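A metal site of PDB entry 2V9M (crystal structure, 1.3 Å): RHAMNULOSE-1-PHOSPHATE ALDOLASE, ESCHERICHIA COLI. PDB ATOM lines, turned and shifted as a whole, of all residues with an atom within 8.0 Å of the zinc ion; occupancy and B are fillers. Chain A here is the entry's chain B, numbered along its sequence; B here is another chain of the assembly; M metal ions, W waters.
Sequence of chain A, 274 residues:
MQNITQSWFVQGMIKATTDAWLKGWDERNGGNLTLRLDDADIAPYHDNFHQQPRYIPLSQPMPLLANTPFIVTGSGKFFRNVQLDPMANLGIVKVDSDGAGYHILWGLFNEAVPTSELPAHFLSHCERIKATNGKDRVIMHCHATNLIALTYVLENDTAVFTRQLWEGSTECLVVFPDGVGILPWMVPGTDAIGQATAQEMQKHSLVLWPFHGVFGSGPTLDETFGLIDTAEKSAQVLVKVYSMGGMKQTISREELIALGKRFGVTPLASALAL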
ATOM      1  N   TRP A  25      13.176   8.171  -0.099  1.00  0.00           N
ATOM      2  CA  TRP A  25      13.066   9.495   0.522  1.00  0.00           C
ATOM      3  C   TRP A  25      13.578  10.605  -0.372  1.00  0.00           C
ATOM      4  O   TRP A  25      13.504  11.762   0.052  1.00  0.00           O
ATOM      5  CB  TRP A  25      13.866   9.520   1.830  1.00  0.00           C
ATOM      6  CG  TRP A  25      13.439   8.539   2.886  1.00  0.00           C
ATOM      7  CD1 TRP A  25      12.288   7.803   2.958  1.00  0.00           C
ATOM      8  CD2 TRP A  25      14.232   8.189   4.025  1.00  0.00           C
ATOM      9  NE1 TRP A  25      12.301   7.015   4.092  1.00  0.00           N
ATOM     10  CE2 TRP A  25      13.504   7.230   4.770  1.00  0.00           C
ATOM     11  CE3 TRP A  25      15.509   8.590   4.490  1.00  0.00           C
ATOM     12  CZ2 TRP A  25      13.999   6.687   5.936  1.00  0.00           C
ATOM     13  CZ3 TRP A  25      16.004   8.057   5.652  1.00  0.00           C
ATOM     14  CH2 TRP A  25      15.254   7.101   6.357  1.00  0.00           C
ATOM     15  N   ASP A  26      14.174  10.302  -1.527  1.00  0.00           N
ATOM     16  CA  ASP A  26      14.925  11.334  -2.259  1.00  0.00           C
ATOM     17  C   ASP A  26      14.773  11.186  -3.773  1.00  0.00           C
ATOM     18  O   ASP A  26      15.738  10.993  -4.510  1.00  0.00           O
ATOM     19  CB  ASP A  26      16.405  11.367  -1.819  1.00  0.00           C
ATOM     20  CG  ASP A  26      16.531  11.842  -0.400  1.00  0.00           C
ATOM     21  OD1 ASP A  26      16.585  10.966   0.494  1.00  0.00           O
ATOM     22  OD2 ASP A  26      16.472  13.090  -0.163  1.00  0.00           O
ATOM     23  N   GLU A  27      13.530  11.292  -4.221  1.00  0.00           N
ATOM     24  CA  GLU A  27      13.200  11.420  -5.626  1.00  0.00           C
ATOM     25  C   GLU A  27      13.931  12.639  -6.227  1.00  0.00           C
ATOM     26  O   GLU A  27      14.095  13.670  -5.544  1.00  0.00           O
ATOM     27  CB  GLU A  27      11.678  11.606  -5.796  1.00  0.00           C
ATOM     28  CG  GLU A  27      11.081  12.880  -5.244  1.00  0.00           C
ATOM     29  CD  GLU A  27      10.830  12.971  -3.762  1.00  0.00           C
ATOM     30  OE1 GLU A  27      10.246  14.020  -3.331  1.00  0.00           O
ATOM     31  OE2 GLU A  27      11.141  12.048  -3.008  1.00  0.00           O
ATOM     32  N   ASN A  29      16.011  15.592  -7.280  1.00  0.00           N
ATOM     33  CA  ASN A  29      17.013  16.291  -6.492  1.00  0.00           C
ATOM     34  C   ASN A  29      16.532  16.613  -5.096  1.00  0.00           C
ATOM     35  O   ASN A  29      17.132  17.435  -4.406  1.00  0.00           O
ATOM     36  CB  ASN A  29      17.454  17.565  -7.195  1.00  0.00           C
ATOM     37  CG  ASN A  29      16.316  18.576  -7.306  1.00  0.00           C
ATOM     38  OD1 ASN A  29      15.265  18.192  -7.688  1.00  0.00           O
ATOM     39  ND2 ASN A  29      16.531  19.837  -6.969  1.00  0.00           N
ATOM     40  N   GLY A  30      15.481  15.938  -4.628  1.00  0.00           N
ATOM     41  CA  GLY A  30      14.930  16.203  -3.304  1.00  0.00           C
ATOM     42  C   GLY A  30      15.884  15.753  -2.223  1.00  0.00           C
ATOM     43  O   GLY A  30      16.506  14.669  -2.314  1.00  0.00           O
ATOM     44  N   GLY A  31      16.063  16.609  -1.228  1.00  0.00           N
ATOM     45  CA  GLY A  31      16.932  16.350  -0.122  1.00  0.00           C
ATOM     46  C   GLY A  31      18.323  16.909  -0.320  1.00  0.00           C
ATOM     47  O   GLY A  31      18.755  17.315  -1.388  1.00  0.00           O
ATOM     48  N   ASN A  32      19.049  17.027   0.792  1.00  0.00           N
ATOM     49  CA  ASN A  32      20.378  17.617   0.810  1.00  0.00           C
ATOM     50  C   ASN A  32      21.071  17.210   2.084  1.00  0.00           C
ATOM     51  O   ASN A  32      20.438  16.921   3.110  1.00  0.00           O
ATOM     52  CB  ASN A  32      20.351  19.137   0.605  1.00  0.00           C
ATOM     53  CG  ASN A  32      19.060  19.817   0.937  1.00  0.00           C
ATOM     54  OD1 ASN A  32      18.775  19.975   2.098  1.00  0.00           O
ATOM     55  ND2 ASN A  32      18.231  20.105  -0.069  1.00  0.00           N
ATOM     56  N   GLU A 117      19.608  24.601  -0.467  1.00  0.00           N
ATOM     57  CA  GLU A 117      19.091  24.765   0.905  1.00  0.00           C
ATOM     58  C   GLU A 117      20.295  25.080   1.810  1.00  0.00           C
ATOM     59  O   GLU A 117      20.214  24.883   3.036  1.00  0.00           O
ATOM     60  CB  GLU A 117      18.340  23.607   1.532  1.00  0.00           C
ATOM     61  CG  GLU A 117      16.952  23.235   1.066  1.00  0.00           C
ATOM     62  CD  GLU A 117      15.957  24.347   0.887  1.00  0.00           C
ATOM     63  OE1 GLU A 117      15.062  24.217   0.027  1.00  0.00           O
ATOM     64  OE2 GLU A 117      16.024  25.359   1.587  1.00  0.00           O
ATOM     65  N   HIS A 141      18.537  16.716   5.222  1.00  0.00           N
ATOM     66  CA  HIS A 141      17.160  16.936   4.776  1.00  0.00           C
ATOM     67  C   HIS A 141      16.775  15.846   3.788  1.00  0.00           C
ATOM     68  O   HIS A 141      17.517  15.582   2.849  1.00  0.00           O
ATOM     69  CB  HIS A 141      16.999  18.310   4.137  1.00  0.00           C
ATOM     70  CG  HIS A 141      15.682  18.492   3.440  1.00  0.00           C
ATOM     71  ND1 HIS A 141      14.446  18.337   4.005  1.00  0.00           N
ATOM     72  CD2 HIS A 141      15.430  18.853   2.160  1.00  0.00           C
ATOM     73  CE1 HIS A 141      13.499  18.573   3.078  1.00  0.00           C
ATOM     74  NE2 HIS A 141      14.058  18.917   1.912  1.00  0.00           N
ATOM     75  N   CYS A 142      15.603  15.234   4.000  1.00  0.00           N
ATOM     76  CA  CYS A 142      15.084  14.295   3.019  1.00  0.00           C
ATOM     77  C   CYS A 142      13.564  14.330   3.035  1.00  0.00           C
ATOM     78  O   CYS A 142      12.942  14.948   3.907  1.00  0.00           O
ATOM     79  CB  CYS A 142      15.621  12.920   3.285  1.00  0.00           C
ATOM     80  SG  CYS A 142      15.015  12.211   4.779  1.00  0.00           S
ATOM     81  N   HIS A 143      12.996  13.677   2.051  1.00  0.00           N
ATOM     82  CA  HIS A 143      11.544  13.635   1.869  1.00  0.00           C
ATOM     83  C   HIS A 143      10.971  12.321   2.398  1.00  0.00           C
ATOM     84  O   HIS A 143      10.497  11.463   1.658  1.00  0.00           O
ATOM     85  CB  HIS A 143      11.214  13.897   0.396  1.00  0.00           C
ATOM     86  CG  HIS A 143      11.649  15.279  -0.045  1.00  0.00           C
ATOM     87  ND1 HIS A 143      11.489  15.701  -1.350  1.00  0.00           N
ATOM     88  CD2 HIS A 143      12.209  16.323   0.586  1.00  0.00           C
ATOM     89  CE1 HIS A 143      11.949  16.944  -1.477  1.00  0.00           C
ATOM     90  NE2 HIS A 143      12.396  17.387  -0.308  1.00  0.00           N
ATOM     91  N   ILE A 148       5.965  12.820   5.916  1.00  0.00           N
ATOM     92  CA  ILE A 148       5.230  13.747   5.050  1.00  0.00           C
ATOM     93  C   ILE A 148       3.746  13.453   5.095  1.00  0.00           C
ATOM     94  O   ILE A 148       2.921  14.379   5.310  1.00  0.00           O
ATOM     95  CB  ILE A 148       5.761  13.728   3.610  1.00  0.00           C
ATOM     96  CG1 ILE A 148       7.202  14.217   3.521  1.00  0.00           C
ATOM     97  CG2 ILE A 148       4.869  14.539   2.679  1.00  0.00           C
ATOM     98  CD1 ILE A 148       7.887  13.836   2.232  1.00  0.00           C
ATOM     99  N   PRO A 188      10.363  27.022   0.161  1.00  0.00           N
ATOM    100  CA  PRO A 188      11.732  26.527   0.328  1.00  0.00           C
ATOM    101  C   PRO A 188      12.794  27.395  -0.352  1.00  0.00           C
ATOM    102  O   PRO A 188      12.535  28.121  -1.295  1.00  0.00           O
ATOM    103  CB  PRO A 188      11.700  25.160  -0.328  1.00  0.00           C
ATOM    104  CG  PRO A 188      10.369  24.924  -0.852  1.00  0.00           C
ATOM    105  CD  PRO A 188       9.528  26.123  -0.660  1.00  0.00           C
ATOM    106  N   TRP A 209       9.008  20.081   7.978  1.00  0.00           N
ATOM    107  CA  TRP A 209       8.484  21.017   6.988  1.00  0.00           C
ATOM    108  C   TRP A 209       7.215  20.385   6.455  1.00  0.00           C
ATOM    109  O   TRP A 209       7.294  19.435   5.658  1.00  0.00           O
ATOM    110  CB  TRP A 209       9.553  21.213   5.909  1.00  0.00           C
ATOM    111  CG  TRP A 209      10.731  22.035   6.253  1.00  0.00           C
ATOM    112  CD1 TRP A 209      11.070  22.623   7.445  1.00  0.00           C
ATOM    113  CD2 TRP A 209      11.772  22.426   5.341  1.00  0.00           C
ATOM    114  NE1 TRP A 209      12.246  23.318   7.346  1.00  0.00           N
ATOM    115  CE2 TRP A 209      12.685  23.223   6.047  1.00  0.00           C
ATOM    116  CE3 TRP A 209      12.010  22.179   3.969  1.00  0.00           C
ATOM    117  CZ2 TRP A 209      13.812  23.778   5.473  1.00  0.00           C
ATOM    118  CZ3 TRP A 209      13.145  22.726   3.359  1.00  0.00           C
ATOM    119  CH2 TRP A 209      14.023  23.516   4.132  1.00  0.00           C
ATOM    120  N   HIS A 212       6.322  18.536   2.925  1.00  0.00           N
ATOM    121  CA  HIS A 212       7.620  18.654   2.279  1.00  0.00           C
ATOM    122  C   HIS A 212       8.571  17.588   2.853  1.00  0.00           C
ATOM    123  O   HIS A 212       9.063  16.747   2.080  1.00  0.00           O
ATOM    124  CB  HIS A 212       8.168  20.100   2.371  1.00  0.00           C
ATOM    125  CG  HIS A 212       9.462  20.330   1.658  1.00  0.00           C
ATOM    126  ND1 HIS A 212       9.910  21.578   1.327  1.00  0.00           N
ATOM    127  CD2 HIS A 212      10.474  19.514   1.206  1.00  0.00           C
ATOM    128  CE1 HIS A 212      11.088  21.455   0.725  1.00  0.00           C
ATOM    129  NE2 HIS A 212      11.485  20.198   0.642  1.00  0.00           N
ATOM    130  N   GLY A 213       8.982  17.689   4.104  1.00  0.00           N
ATOM    131  CA  GLY A 213       9.946  16.697   4.562  1.00  0.00           C
ATOM    132  C   GLY A 213      10.496  17.026   5.936  1.00  0.00           C
ATOM    133  O   GLY A 213       9.825  17.684   6.727  1.00  0.00           O
ATOM    134  N   VAL A 214      11.697  16.497   6.208  1.00  0.00           N
ATOM    135  CA  VAL A 214      12.275  16.532   7.526  1.00  0.00           C
ATOM    136  C   VAL A 214      13.715  17.032   7.456  1.00  0.00           C
ATOM    137  O   VAL A 214      14.401  16.842   6.457  1.00  0.00           O
ATOM    138  CB  VAL A 214      12.174  15.155   8.189  1.00  0.00           C
ATOM    139  CG1 VAL A 214      13.047  14.154   7.483  1.00  0.00           C
ATOM    140  CG2 VAL A 214      12.475  15.162   9.671  1.00  0.00           C
ATOM    141  N   PHE A 215      14.133  17.646   8.539  1.00  0.00           N
ATOM    142  CA  PHE A 215      15.504  18.060   8.786  1.00  0.00           C
ATOM    143  C   PHE A 215      15.984  17.455  10.088  1.00  0.00           C
ATOM    144  O   PHE A 215      15.248  17.550  11.073  1.00  0.00           O
ATOM    145  CB  PHE A 215      15.702  19.555   8.963  1.00  0.00           C
ATOM    146  CG  PHE A 215      16.085  20.293   7.724  1.00  0.00           C
ATOM    147  CD1 PHE A 215      15.028  20.371   6.807  1.00  0.00           C
ATOM    148  CD2 PHE A 215      17.243  20.808   7.374  1.00  0.00           C
ATOM    149  CE1 PHE A 215      15.381  20.958   5.622  1.00  0.00           C
ATOM    150  CE2 PHE A 215      17.631  21.460   6.249  1.00  0.00           C
ATOM    151  CZ  PHE A 215      16.575  21.556   5.322  1.00  0.00           C
ATOM    152  N   THR B 170       5.639  19.392  -1.873  1.00  0.00           N
ATOM    153  CA  THR B 170       5.846  20.813  -2.146  1.00  0.00           C
ATOM    154  C   THR B 170       6.480  21.069  -3.507  1.00  0.00           C
ATOM    155  O   THR B 170       6.099  21.997  -4.220  1.00  0.00           O
ATOM    156  CB  THR B 170       6.664  21.458  -1.018  1.00  0.00           C
ATOM    157  OG1 THR B 170       5.795  21.612   0.143  1.00  0.00           O
ATOM    158  CG2 THR B 170       7.171  22.848  -1.374  1.00  0.00           C
ATOM    159  N   GLU B 171       7.492  20.286  -3.855  1.00  0.00           N
ATOM    160  CA  GLU B 171       8.247  20.421  -5.087  1.00  0.00           C
ATOM    161  C   GLU B 171       7.412  20.259  -6.334  1.00  0.00           C
ATOM    162  O   GLU B 171       7.801  20.712  -7.406  1.00  0.00           O
ATOM    163  CB  GLU B 171       9.364  19.357  -5.098  1.00  0.00           C
ATOM    164  CG  GLU B 171       8.758  17.949  -5.231  1.00  0.00           C
ATOM    165  CD  GLU B 171       9.613  16.794  -4.750  1.00  0.00           C
ATOM    166  OE1 GLU B 171      10.785  16.929  -4.538  1.00  0.00           O
ATOM    167  OE2 GLU B 171       9.036  15.729  -4.624  1.00  0.00           O
HETATM  168 ZN    ZN M   1      13.119  19.231   0.120  1.00  0.00          ZN
HETATM  169  O   HOH W   1      11.944  19.982  -2.032  1.00  0.00           O
HETATM  170  O   HOH W   2      14.828  19.592  -1.139  1.00  0.00           O
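A ring nitrogen (ND1) of His 143 sits close to the side-chain carboxylate of Glu 171 of chain B, 3.5 Å away. The side-chain carboxylate of Glu 27 lies within hydrogen-bond range of a ring nitrogen (ND1) of His 143. The backbone NH (N) of His 143 sits at hydrogen-bond distance from the backbone carbonyl oxygen (O) of Trp 25 (2.8 Å). The backbone carbonyl oxygen (O) of Asn 32 is in hydrogen-bond range of the backbone NH (N) of His 141, 2.8 Å away. The backbone carbonyl oxygen of Val 214 is in hydrogen-bond range of a ring nitrogen (ND1) of His 141.
The zinc ion is bound by a ring nitrogen (NE2) of His 212, a ring nitrogen (NE2) of His 143, a ring nitrogen (NE2) of His 141, water W2 and water W1.
Three residues have an atom within 4 Å of the zinc ion: His 141, His 143 and His 212. The nearest printed residue that does not touch the zinc ion is Gly 31 (4.2 Å).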
